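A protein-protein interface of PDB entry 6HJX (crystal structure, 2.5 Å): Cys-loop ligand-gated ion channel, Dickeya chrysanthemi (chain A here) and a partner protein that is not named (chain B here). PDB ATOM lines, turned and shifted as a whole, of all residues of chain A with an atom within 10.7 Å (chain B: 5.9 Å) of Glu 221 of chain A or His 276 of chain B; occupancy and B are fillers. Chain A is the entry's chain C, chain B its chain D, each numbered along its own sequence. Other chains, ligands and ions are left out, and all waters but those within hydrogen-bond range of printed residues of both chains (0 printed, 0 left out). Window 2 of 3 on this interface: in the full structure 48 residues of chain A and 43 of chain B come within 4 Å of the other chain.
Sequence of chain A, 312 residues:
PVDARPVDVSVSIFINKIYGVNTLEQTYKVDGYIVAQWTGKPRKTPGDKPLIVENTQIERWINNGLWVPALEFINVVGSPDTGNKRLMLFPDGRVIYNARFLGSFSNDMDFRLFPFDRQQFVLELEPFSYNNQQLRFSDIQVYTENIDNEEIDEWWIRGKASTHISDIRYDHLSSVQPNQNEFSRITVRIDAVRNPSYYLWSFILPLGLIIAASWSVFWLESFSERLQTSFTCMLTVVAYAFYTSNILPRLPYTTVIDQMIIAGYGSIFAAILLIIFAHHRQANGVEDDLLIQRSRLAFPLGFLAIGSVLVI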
ATOM      1  N   SER A 216      13.029   1.530 -21.390  1.00  0.00           N
ATOM      2  CA  SER A 216      13.969   0.476 -21.037  1.00  0.00           C
ATOM      3  C   SER A 216      13.360  -0.917 -21.114  1.00  0.00           C
ATOM      4  O   SER A 216      14.094  -1.900 -20.961  1.00  0.00           O
ATOM      5  CB  SER A 216      14.517   0.708 -19.628  1.00  0.00           C
ATOM      6  OG  SER A 216      13.544   0.405 -18.647  1.00  0.00           O
ATOM      7  N   VAL A 217      12.048  -1.034 -21.340  1.00  0.00           N
ATOM      8  CA  VAL A 217      11.434  -2.350 -21.466  1.00  0.00           C
ATOM      9  C   VAL A 217      11.999  -3.111 -22.656  1.00  0.00           C
ATOM     10  O   VAL A 217      11.955  -4.346 -22.680  1.00  0.00           O
ATOM     11  CB  VAL A 217       9.898  -2.234 -21.583  1.00  0.00           C
ATOM     12  CG1 VAL A 217       9.318  -1.554 -20.354  1.00  0.00           C
ATOM     13  CG2 VAL A 217       9.503  -1.494 -22.856  1.00  0.00           C
ATOM     14  N   PHE A 218      12.526  -2.400 -23.655  1.00  0.00           N
ATOM     15  CA  PHE A 218      13.104  -3.050 -24.824  1.00  0.00           C
ATOM     16  C   PHE A 218      14.407  -3.767 -24.505  1.00  0.00           C
ATOM     17  O   PHE A 218      14.851  -4.605 -25.297  1.00  0.00           O
ATOM     18  CB  PHE A 218      13.334  -2.013 -25.924  1.00  0.00           C
ATOM     19  CG  PHE A 218      12.079  -1.325 -26.376  1.00  0.00           C
ATOM     20  CD1 PHE A 218      10.954  -2.061 -26.706  1.00  0.00           C
ATOM     21  CD2 PHE A 218      12.018   0.055 -26.458  1.00  0.00           C
ATOM     22  CE1 PHE A 218       9.794  -1.437 -27.118  1.00  0.00           C
ATOM     23  CE2 PHE A 218      10.858   0.685 -26.870  1.00  0.00           C
ATOM     24  CZ  PHE A 218       9.745  -0.063 -27.200  1.00  0.00           C
ATOM     25  N   TRP A 219      15.027  -3.462 -23.368  1.00  0.00           N
ATOM     26  CA  TRP A 219      16.281  -4.083 -22.970  1.00  0.00           C
ATOM     27  C   TRP A 219      16.083  -5.335 -22.125  1.00  0.00           C
ATOM     28  O   TRP A 219      17.070  -5.900 -21.642  1.00  0.00           O
ATOM     29  CB  TRP A 219      17.138  -3.075 -22.200  1.00  0.00           C
ATOM     30  CG  TRP A 219      17.513  -1.875 -23.010  1.00  0.00           C
ATOM     31  CD1 TRP A 219      16.720  -0.804 -23.302  1.00  0.00           C
ATOM     32  CD2 TRP A 219      18.776  -1.620 -23.633  1.00  0.00           C
ATOM     33  NE1 TRP A 219      17.410   0.102 -24.070  1.00  0.00           N
ATOM     34  CE2 TRP A 219      18.676  -0.374 -24.286  1.00  0.00           C
ATOM     35  CE3 TRP A 219      19.982  -2.323 -23.702  1.00  0.00           C
ATOM     36  CZ2 TRP A 219      19.734   0.180 -25.000  1.00  0.00           C
ATOM     37  CZ3 TRP A 219      21.032  -1.769 -24.411  1.00  0.00           C
ATOM     38  CH2 TRP A 219      20.902  -0.530 -25.049  1.00  0.00           C
ATOM     39  N   LEU A 220      14.844  -5.774 -21.925  1.00  0.00           N
ATOM     40  CA  LEU A 220      14.576  -7.013 -21.210  1.00  0.00           C
ATOM     41  C   LEU A 220      14.610  -8.188 -22.178  1.00  0.00           C
ATOM     42  O   LEU A 220      14.227  -8.072 -23.345  1.00  0.00           O
ATOM     43  CB  LEU A 220      13.223  -6.950 -20.499  1.00  0.00           C
ATOM     44  CG  LEU A 220      13.160  -6.020 -19.284  1.00  0.00           C
ATOM     45  CD1 LEU A 220      11.720  -5.766 -18.870  1.00  0.00           C
ATOM     46  CD2 LEU A 220      13.956  -6.595 -18.118  1.00  0.00           C
ATOM     47  N   GLU A 221      15.070  -9.328 -21.675  1.00  0.00           N
ATOM     48  CA  GLU A 221      15.389 -10.490 -22.507  1.00  0.00           C
ATOM     49  C   GLU A 221      14.318 -11.569 -22.402  1.00  0.00           C
ATOM     50  O   GLU A 221      14.618 -12.752 -22.241  1.00  0.00           O
ATOM     51  CB  GLU A 221      16.757 -11.037 -22.115  1.00  0.00           C
ATOM     52  CG  GLU A 221      17.899 -10.050 -22.339  1.00  0.00           C
ATOM     53  CD  GLU A 221      19.069 -10.268 -21.396  1.00  0.00           C
ATOM     54  OE1 GLU A 221      18.855 -10.784 -20.277  1.00  0.00           O
ATOM     55  OE2 GLU A 221      20.206  -9.917 -21.772  1.00  0.00           O
ATOM     56  N   SER A 222      13.051 -11.172 -22.503  1.00  0.00           N
ATOM     57  CA  SER A 222      11.940 -12.111 -22.433  1.00  0.00           C
ATOM     58  C   SER A 222      10.643 -11.365 -22.708  1.00  0.00           C
ATOM     59  O   SER A 222      10.431 -10.271 -22.179  1.00  0.00           O
ATOM     60  CB  SER A 222      11.872 -12.792 -21.060  1.00  0.00           C
ATOM     61  OG  SER A 222      10.765 -13.673 -20.985  1.00  0.00           O
ATOM     62  N   PHE A 223       9.778 -11.970 -23.525  1.00  0.00           N
ATOM     63  CA  PHE A 223       8.472 -11.375 -23.798  1.00  0.00           C
ATOM     64  C   PHE A 223       7.697 -11.137 -22.508  1.00  0.00           C
ATOM     65  O   PHE A 223       7.123 -10.061 -22.302  1.00  0.00           O
ATOM     66  CB  PHE A 223       7.675 -12.276 -24.743  1.00  0.00           C
ATOM     67  CG  PHE A 223       6.214 -11.930 -24.821  1.00  0.00           C
ATOM     68  CD1 PHE A 223       5.773 -10.910 -25.646  1.00  0.00           C
ATOM     69  CD2 PHE A 223       5.283 -12.630 -24.072  1.00  0.00           C
ATOM     70  CE1 PHE A 223       4.430 -10.591 -25.719  1.00  0.00           C
ATOM     71  CE2 PHE A 223       3.939 -12.316 -24.142  1.00  0.00           C
ATOM     72  CZ  PHE A 223       3.513 -11.295 -24.967  1.00  0.00           C
ATOM     73  N   SER A 224       7.665 -12.138 -21.626  1.00  0.00           N
ATOM     74  CA  SER A 224       6.928 -11.999 -20.374  1.00  0.00           C
ATOM     75  C   SER A 224       7.409 -10.784 -19.591  1.00  0.00           C
ATOM     76  O   SER A 224       6.602 -10.000 -19.078  1.00  0.00           O
ATOM     77  CB  SER A 224       7.078 -13.269 -19.537  1.00  0.00           C
ATOM     78  OG  SER A 224       6.481 -13.107 -18.264  1.00  0.00           O
ATOM     79  N   GLU A 225       8.728 -10.612 -19.494  1.00  0.00           N
ATOM     80  CA  GLU A 225       9.282  -9.486 -18.751  1.00  0.00           C
ATOM     81  C   GLU A 225       8.973  -8.162 -19.437  1.00  0.00           C
ATOM     82  O   GLU A 225       8.753  -7.146 -18.766  1.00  0.00           O
ATOM     83  CB  GLU A 225      10.792  -9.657 -18.594  1.00  0.00           C
ATOM     84  CG  GLU A 225      11.197 -10.807 -17.691  1.00  0.00           C
ATOM     85  CD  GLU A 225      12.677 -11.118 -17.778  1.00  0.00           C
ATOM     86  OE1 GLU A 225      13.045 -12.084 -18.475  1.00  0.00           O
ATOM     87  OE2 GLU A 225      13.476 -10.387 -17.160  1.00  0.00           O
ATOM     88  N   ARG A 226       8.966  -8.148 -20.771  1.00  0.00           N
ATOM     89  CA  ARG A 226       8.727  -6.904 -21.494  1.00  0.00           C
ATOM     90  C   ARG A 226       7.283  -6.442 -21.335  1.00  0.00           C
ATOM     91  O   ARG A 226       7.027  -5.250 -21.132  1.00  0.00           O
ATOM     92  CB  ARG A 226       9.075  -7.078 -22.973  1.00  0.00           C
ATOM     93  CG  ARG A 226      10.563  -7.249 -23.244  1.00  0.00           C
ATOM     94  CD  ARG A 226      10.901  -7.121 -24.727  1.00  0.00           C
ATOM     95  NE  ARG A 226      10.321  -8.191 -25.537  1.00  0.00           N
ATOM     96  CZ  ARG A 226      10.913  -9.357 -25.788  1.00  0.00           C
ATOM     97  NH1 ARG A 226      12.114  -9.626 -25.291  1.00  0.00           N
ATOM     98  NH2 ARG A 226      10.298 -10.259 -26.540  1.00  0.00           N
ATOM     99  N   LEU A 227       6.330  -7.372 -21.420  1.00  0.00           N
ATOM    100  CA  LEU A 227       4.920  -7.006 -21.362  1.00  0.00           C
ATOM    101  C   LEU A 227       4.464  -6.696 -19.942  1.00  0.00           C
ATOM    102  O   LEU A 227       3.608  -5.825 -19.752  1.00  0.00           O
ATOM    103  CB  LEU A 227       4.066  -8.130 -21.953  1.00  0.00           C
ATOM    104  CG  LEU A 227       2.565  -7.863 -22.091  1.00  0.00           C
ATOM    105  CD1 LEU A 227       2.299  -6.680 -23.009  1.00  0.00           C
ATOM    106  CD2 LEU A 227       1.853  -9.104 -22.607  1.00  0.00           C
ATOM    107  N   GLN A 228       5.018  -7.381 -18.940  1.00  0.00           N
ATOM    108  CA  GLN A 228       4.594  -7.152 -17.562  1.00  0.00           C
ATOM    109  C   GLN A 228       5.149  -5.838 -17.024  1.00  0.00           C
ATOM    110  O   GLN A 228       4.425  -5.057 -16.395  1.00  0.00           O
ATOM    111  CB  GLN A 228       5.029  -8.321 -16.678  1.00  0.00           C
ATOM    112  CG  GLN A 228       4.251  -9.603 -16.927  1.00  0.00           C
ATOM    113  CD  GLN A 228       4.688 -10.737 -16.022  1.00  0.00           C
ATOM    114  OE1 GLN A 228       5.820 -10.756 -15.531  1.00  0.00           O
ATOM    115  NE2 GLN A 228       3.791 -11.689 -15.793  1.00  0.00           N
ATOM    116  N   THR A 229       6.439  -5.577 -17.253  1.00  0.00           N
ATOM    117  CA  THR A 229       7.031  -4.327 -16.789  1.00  0.00           C
ATOM    118  C   THR A 229       6.348  -3.121 -17.420  1.00  0.00           C
ATOM    119  O   THR A 229       6.251  -2.062 -16.788  1.00  0.00           O
ATOM    120  CB  THR A 229       8.531  -4.310 -17.095  1.00  0.00           C
ATOM    121  OG1 THR A 229       9.163  -5.433 -16.470  1.00  0.00           O
ATOM    122  CG2 THR A 229       9.179  -3.025 -16.587  1.00  0.00           C
ATOM    123  N   ILE A 275       5.500  -5.088 -28.504  1.00  0.00           N
ATOM    124  CA  ILE A 275       5.993  -6.264 -27.790  1.00  0.00           C
ATOM    125  C   ILE A 275       5.192  -7.501 -28.176  1.00  0.00           C
ATOM    126  O   ILE A 275       5.750  -8.595 -28.337  1.00  0.00           O
ATOM    127  CB  ILE A 275       5.956  -6.010 -26.270  1.00  0.00           C
ATOM    128  CG1 ILE A 275       7.020  -4.980 -25.887  1.00  0.00           C
ATOM    129  CG2 ILE A 275       6.162  -7.304 -25.493  1.00  0.00           C
ATOM    130  CD1 ILE A 275       6.849  -4.412 -24.499  1.00  0.00           C
ATOM    131  N   HIS A 279       6.407 -10.843 -30.872  1.00  0.00           N
ATOM    132  CA  HIS A 279       6.455 -12.184 -30.303  1.00  0.00           C
ATOM    133  C   HIS A 279       5.418 -13.120 -30.914  1.00  0.00           C
ATOM    134  O   HIS A 279       5.642 -14.335 -30.951  1.00  0.00           O
ATOM    135  CB  HIS A 279       6.252 -12.108 -28.788  1.00  0.00           C
ATOM    136  CG  HIS A 279       6.211 -13.443 -28.115  1.00  0.00           C
ATOM    137  ND1 HIS A 279       5.048 -14.169 -27.973  1.00  0.00           N
ATOM    138  CD2 HIS A 279       7.191 -14.184 -27.545  1.00  0.00           C
ATOM    139  CE1 HIS A 279       5.313 -15.301 -27.345  1.00  0.00           C
ATOM    140  NE2 HIS A 279       6.606 -15.334 -27.073  1.00  0.00           N
ATOM    141  N   ASP A 289      11.924 -12.754 -33.132  1.00  0.00           N
ATOM    142  CA  ASP A 289      11.272 -11.839 -32.201  1.00  0.00           C
ATOM    143  C   ASP A 289      12.288 -10.910 -31.544  1.00  0.00           C
ATOM    144  O   ASP A 289      12.126  -9.686 -31.554  1.00  0.00           O
ATOM    145  CB  ASP A 289      10.505 -12.637 -31.146  1.00  0.00           C
ATOM    146  CG  ASP A 289      10.071 -11.784 -29.969  1.00  0.00           C
ATOM    147  OD1 ASP A 289       9.309 -10.817 -30.180  1.00  0.00           O
ATOM    148  OD2 ASP A 289      10.490 -12.083 -28.831  1.00  0.00           O
ATOM    149  N   LEU A 290      13.354 -11.481 -30.975  1.00  0.00           N
ATOM    150  CA  LEU A 290      14.332 -10.686 -30.241  1.00  0.00           C
ATOM    151  C   LEU A 290      15.028  -9.651 -31.116  1.00  0.00           C
ATOM    152  O   LEU A 290      15.565  -8.672 -30.585  1.00  0.00           O
ATOM    153  CB  LEU A 290      15.375 -11.607 -29.605  1.00  0.00           C
ATOM    154  N   LEU A 291      15.036  -9.833 -32.438  1.00  0.00           N
ATOM    155  CA  LEU A 291      15.785  -8.920 -33.295  1.00  0.00           C
ATOM    156  C   LEU A 291      15.039  -7.606 -33.507  1.00  0.00           C
ATOM    157  O   LEU A 291      15.658  -6.536 -33.506  1.00  0.00           O
ATOM    158  CB  LEU A 291      16.086  -9.584 -34.640  1.00  0.00           C
ATOM    159  CG  LEU A 291      17.168  -8.898 -35.480  1.00  0.00           C
ATOM    160  CD1 LEU A 291      18.546  -9.038 -34.838  1.00  0.00           C
ATOM    161  CD2 LEU A 291      17.184  -9.451 -36.897  1.00  0.00           C
ATOM    162  N   GLN A 293      12.905  -6.489 -31.363  1.00  0.00           N
ATOM    163  CA  GLN A 293      12.987  -5.883 -30.041  1.00  0.00           C
ATOM    164  C   GLN A 293      14.263  -5.074 -29.855  1.00  0.00           C
ATOM    165  O   GLN A 293      14.370  -4.338 -28.867  1.00  0.00           O
ATOM    166  CB  GLN A 293      12.902  -6.958 -28.960  1.00  0.00           C
ATOM    167  CG  GLN A 293      11.589  -7.720 -28.939  1.00  0.00           C
ATOM    168  CD  GLN A 293      10.379  -6.834 -28.698  1.00  0.00           C
ATOM    169  OE1 GLN A 293       9.270  -7.172 -29.106  1.00  0.00           O
ATOM    170  NE2 GLN A 293      10.582  -5.705 -28.024  1.00  0.00           N
ATOM    171  N   ARG A 294      15.224  -5.183 -30.773  1.00  0.00           N
ATOM    172  CA  ARG A 294      16.406  -4.331 -30.755  1.00  0.00           C
ATOM    173  C   ARG A 294      16.084  -2.966 -31.356  1.00  0.00           C
ATOM    174  O   ARG A 294      16.954  -2.321 -31.949  1.00  0.00           O
ATOM    175  CB  ARG A 294      17.557  -4.995 -31.511  1.00  0.00           C
ATOM    176  N   ARG A 296      15.574  -0.526 -29.491  1.00  0.00           N
ATOM    177  CA  ARG A 296      15.814   0.308 -28.319  1.00  0.00           C
ATOM    178  C   ARG A 296      16.126   1.746 -28.711  1.00  0.00           C
ATOM    179  O   ARG A 296      15.848   2.674 -27.943  1.00  0.00           O
ATOM    180  CB  ARG A 296      16.959  -0.288 -27.495  1.00  0.00           C
ATOM    181  CG  ARG A 296      16.729  -1.742 -27.086  1.00  0.00           C
ATOM    182  CD  ARG A 296      18.031  -2.528 -27.017  1.00  0.00           C
ATOM    183  NE  ARG A 296      17.804  -3.935 -26.701  1.00  0.00           N
ATOM    184  CZ  ARG A 296      18.770  -4.826 -26.502  1.00  0.00           C
ATOM    185  NH1 ARG A 296      20.042  -4.464 -26.580  1.00  0.00           N
ATOM    186  NH2 ARG A 296      18.462  -6.084 -26.218  1.00  0.00           N
ATOM    187  N   PHE B 220      20.372  -9.439 -13.769  1.00  0.00           N
ATOM    188  CA  PHE B 220      20.003  -8.223 -14.487  1.00  0.00           C
ATOM    189  C   PHE B 220      18.492  -8.086 -14.609  1.00  0.00           C
ATOM    190  O   PHE B 220      17.970  -6.966 -14.658  1.00  0.00           O
ATOM    191  CB  PHE B 220      20.643  -8.218 -15.876  1.00  0.00           C
ATOM    192  CG  PHE B 220      19.936  -7.332 -16.863  1.00  0.00           C
ATOM    193  CD1 PHE B 220      20.193  -5.972 -16.904  1.00  0.00           C
ATOM    194  CD2 PHE B 220      19.008  -7.859 -17.748  1.00  0.00           C
ATOM    195  CE1 PHE B 220      19.539  -5.154 -17.807  1.00  0.00           C
ATOM    196  CE2 PHE B 220      18.352  -7.047 -18.653  1.00  0.00           C
ATOM    197  CZ  PHE B 220      18.619  -5.694 -18.683  1.00  0.00           C
ATOM    198  N   ARG B 223      17.247  -6.761 -11.082  1.00  0.00           N
ATOM    199  CA  ARG B 223      17.677  -5.404 -10.760  1.00  0.00           C
ATOM    200  C   ARG B 223      16.867  -4.372 -11.533  1.00  0.00           C
ATOM    201  O   ARG B 223      16.407  -3.374 -10.965  1.00  0.00           O
ATOM    202  CB  ARG B 223      19.170  -5.245 -11.051  1.00  0.00           C
ATOM    203  CG  ARG B 223      20.040  -6.262 -10.328  1.00  0.00           C
ATOM    204  CD  ARG B 223      21.513  -5.881 -10.350  1.00  0.00           C
ATOM    205  NE  ARG B 223      22.221  -6.439 -11.500  1.00  0.00           N
ATOM    206  CZ  ARG B 223      22.669  -7.690 -11.570  1.00  0.00           C
ATOM    207  NH1 ARG B 223      22.477  -8.528 -10.560  1.00  0.00           N
ATOM    208  NH2 ARG B 223      23.305  -8.107 -12.655  1.00  0.00           N
ATOM    209  N   LEU B 271      22.855   2.520 -15.174  1.00  0.00           N
ATOM    210  CA  LEU B 271      24.007   1.722 -14.765  1.00  0.00           C
ATOM    211  C   LEU B 271      23.715   0.232 -14.897  1.00  0.00           C
ATOM    212  O   LEU B 271      24.536  -0.529 -15.421  1.00  0.00           O
ATOM    213  CB  LEU B 271      24.398   2.078 -13.331  1.00  0.00           C
ATOM    214  CG  LEU B 271      25.611   1.353 -12.746  1.00  0.00           C
ATOM    215  CD1 LEU B 271      26.410   2.290 -11.855  1.00  0.00           C
ATOM    216  CD2 LEU B 271      25.183   0.122 -11.959  1.00  0.00           C
ATOM    217  N   ILE B 272      22.544  -0.205 -14.427  1.00  0.00           N
ATOM    218  CA  ILE B 272      22.175  -1.614 -14.535  1.00  0.00           C
ATOM    219  C   ILE B 272      22.203  -2.058 -15.994  1.00  0.00           C
ATOM    220  O   ILE B 272      22.728  -3.128 -16.324  1.00  0.00           O
ATOM    221  CB  ILE B 272      20.798  -1.855 -13.892  1.00  0.00           C
ATOM    222  CG1 ILE B 272      20.882  -1.647 -12.375  1.00  0.00           C
ATOM    223  CG2 ILE B 272      20.297  -3.258 -14.196  1.00  0.00           C
ATOM    224  CD1 ILE B 272      19.534  -1.499 -11.702  1.00  0.00           C
ATOM    225  N   ILE B 273      21.637  -1.246 -16.890  1.00  0.00           N
ATOM    226  CA  ILE B 273      21.678  -1.569 -18.313  1.00  0.00           C
ATOM    227  C   ILE B 273      23.101  -1.450 -18.843  1.00  0.00           C
ATOM    228  O   ILE B 273      23.556  -2.285 -19.634  1.00  0.00           O
ATOM    229  CB  ILE B 273      20.700  -0.665 -19.086  1.00  0.00           C
ATOM    230  CG1 ILE B 273      19.256  -1.063 -18.758  1.00  0.00           C
ATOM    231  CG2 ILE B 273      20.953  -0.746 -20.592  1.00  0.00           C
ATOM    232  CD1 ILE B 273      18.204  -0.141 -19.336  1.00  0.00           C
ATOM    233  N   PHE B 274      23.826  -0.413 -18.419  1.00  0.00           N
ATOM    234  CA  PHE B 274      25.201  -0.240 -18.872  1.00  0.00           C
ATOM    235  C   PHE B 274      26.070  -1.417 -18.446  1.00  0.00           C
ATOM    236  O   PHE B 274      26.964  -1.838 -19.188  1.00  0.00           O
ATOM    237  CB  PHE B 274      25.769   1.072 -18.331  1.00  0.00           C
ATOM    238  CG  PHE B 274      27.117   1.426 -18.894  1.00  0.00           C
ATOM    239  CD1 PHE B 274      27.244   1.836 -20.211  1.00  0.00           C
ATOM    240  CD2 PHE B 274      28.255   1.353 -18.108  1.00  0.00           C
ATOM    241  CE1 PHE B 274      28.482   2.162 -20.736  1.00  0.00           C
ATOM    242  CE2 PHE B 274      29.495   1.679 -18.626  1.00  0.00           C
ATOM    243  CZ  PHE B 274      29.609   2.083 -19.941  1.00  0.00           C
ATOM    244  N   ALA B 275      25.818  -1.965 -17.254  1.00  0.00           N
ATOM    245  CA  ALA B 275      26.603  -3.095 -16.774  1.00  0.00           C
ATOM    246  C   ALA B 275      26.317  -4.362 -17.568  1.00  0.00           C
ATOM    247  O   ALA B 275      27.199  -5.216 -17.712  1.00  0.00           O
ATOM    248  CB  ALA B 275      26.324  -3.334 -15.290  1.00  0.00           C
ATOM    249  N   HIS B 276      25.100  -4.503 -18.089  1.00  0.00           N
ATOM    250  CA  HIS B 276      24.688  -5.721 -18.775  1.00  0.00           C
ATOM    251  C   HIS B 276      25.129  -5.768 -20.234  1.00  0.00           C
ATOM    252  O   HIS B 276      24.814  -6.744 -20.923  1.00  0.00           O
ATOM    253  CB  HIS B 276      23.166  -5.866 -18.690  1.00  0.00           C
ATOM    254  CG  HIS B 276      22.661  -7.220 -19.082  1.00  0.00           C
ATOM    255  ND1 HIS B 276      22.780  -8.322 -18.264  1.00  0.00           N
ATOM    256  CD2 HIS B 276      22.035  -7.649 -20.203  1.00  0.00           C
ATOM    257  CE1 HIS B 276      22.249  -9.372 -18.864  1.00  0.00           C
ATOM    258  NE2 HIS B 276      21.791  -8.991 -20.043  1.00  0.00           N
ATOM    259  N   HIS B 277      25.851  -4.746 -20.725  1.00  0.00           N
ATOM    260  CA  HIS B 277      26.264  -4.743 -22.124  1.00  0.00           C
ATOM    261  C   HIS B 277      27.622  -4.079 -22.352  1.00  0.00           C
ATOM    262  O   HIS B 277      27.923  -3.705 -23.492  1.00  0.00           O
ATOM    263  CB  HIS B 277      25.215  -4.026 -22.994  1.00  0.00           C
ATOM    264  CG  HIS B 277      23.874  -4.691 -23.003  1.00  0.00           C
ATOM    265  ND1 HIS B 277      23.516  -5.634 -23.942  1.00  0.00           N
ATOM    266  CD2 HIS B 277      22.800  -4.545 -22.190  1.00  0.00           C
ATOM    267  CE1 HIS B 277      22.282  -6.044 -23.706  1.00  0.00           C
ATOM    268  NE2 HIS B 277      21.825  -5.399 -22.648  1.00  0.00           N
ATOM    269  N   ARG B 278      28.452  -3.928 -21.319  1.00  0.00           N
ATOM    270  CA  ARG B 278      29.708  -3.199 -21.453  1.00  0.00           C
ATOM    271  C   ARG B 278      30.853  -4.076 -21.950  1.00  0.00           C
ATOM    272  O   ARG B 278      31.683  -3.614 -22.739  1.00  0.00           O
ATOM    273  CB  ARG B 278      30.093  -2.567 -20.111  1.00  0.00           C
ATOM    274  N   ASP B 285      28.114  -8.733 -18.299  1.00  0.00           N
ATOM    275  CA  ASP B 285      28.662  -9.580 -17.247  1.00  0.00           C
ATOM    276  C   ASP B 285      29.667  -8.804 -16.404  1.00  0.00           C
ATOM    277  O   ASP B 285      30.695  -9.344 -15.995  1.00  0.00           O
ATOM    278  CB  ASP B 285      29.326 -10.822 -17.847  1.00  0.00           C
ATOM    279  N   ASP B 286      29.362  -7.535 -16.145  1.00  0.00           N
ATOM    280  CA  ASP B 286      30.248  -6.668 -15.372  1.00  0.00           C
ATOM    281  C   ASP B 286      29.742  -6.567 -13.933  1.00  0.00           C
ATOM    282  O   ASP B 286      29.228  -5.541 -13.485  1.00  0.00           O
ATOM    283  CB  ASP B 286      30.351  -5.295 -16.031  1.00  0.00           C
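Of chain B, only Phe 220 (3.9 Å) and His 276 (2.5 Å) come within 4 Å of Glu 221 of chain A.
His 276 of chain B touches one residue of chain A.
Phe 220 of chain B touches two residues of chain A.
No residue of chain A comes within 4 Å of Ala 275 of chain B.
Of chain A, only Trp 219 and Arg 296 come within 4 Å of His 277 of chain B.
No residue of chain A comes within 4 Å of Asp 286 of chain B.
Of the printed residues of chain B, Ser 216 of chain A touches Ile 273 (3.8 Å).
Printed residues of chain B within 4 Å of Trp 219 of chain A: Phe 220 (3.3 Å), Ile 273 (3.6 Å) and His 277 (3.7 Å).
Arg 226 of chain A touches none of the printed residues of chain B.
The nearest residue of chain B that does not touch Glu 221 of chain A is His 277 of chain B (4.8 Å).
The nearest residue of chain A that does not touch His 276 of chain B is Trp 219 of chain A (5.5 Å).
The nearest printed residue of chain A that does not touch Ile 273 of chain B is Val 217 of chain A (6.5 Å).
O of Phe 218 of chain A lies within hydrogen-bond range of NE of Arg 296 of chain A (3.3 Å).
Printed residues of chain A that touch a printed residue of chain B: Ser 216, Trp 219, Glu 221 and Arg 296.
Hydrophobic or aromatic side chains of chain A that line the printed part of chain B: Trp 219.
Of the 12 printed residues of chain B, 4 touch a printed residue of chain A.
Printed residues of chain B that touch a printed residue of chain A: Phe 220, Ile 273, His 276 and His 277.
Among the printed residues, 7 pairs touch across the chains.
Among the printed residues, no Asp or Glu carboxylate lies within 4 Å of a Lys or Arg side-chain nitrogen of the other chain.
Among the printed residues, pairs that only touch across the chains: Trp 219 of chain A with Phe 220 of chain B, Trp 219 of chain A with Ile 273 of chain B, Trp 219 of chain A with His 277 of chain B, Ser 216 of chain A with Ile 273 of chain B, Glu 221 of chain A with Phe 220 of chain B and Arg 296 of chain A with His 277 of chain B.
OE2 of Glu 221 of chain A lies within hydrogen-bond range of NE2 of His 276 of chain B (2.5 Å).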
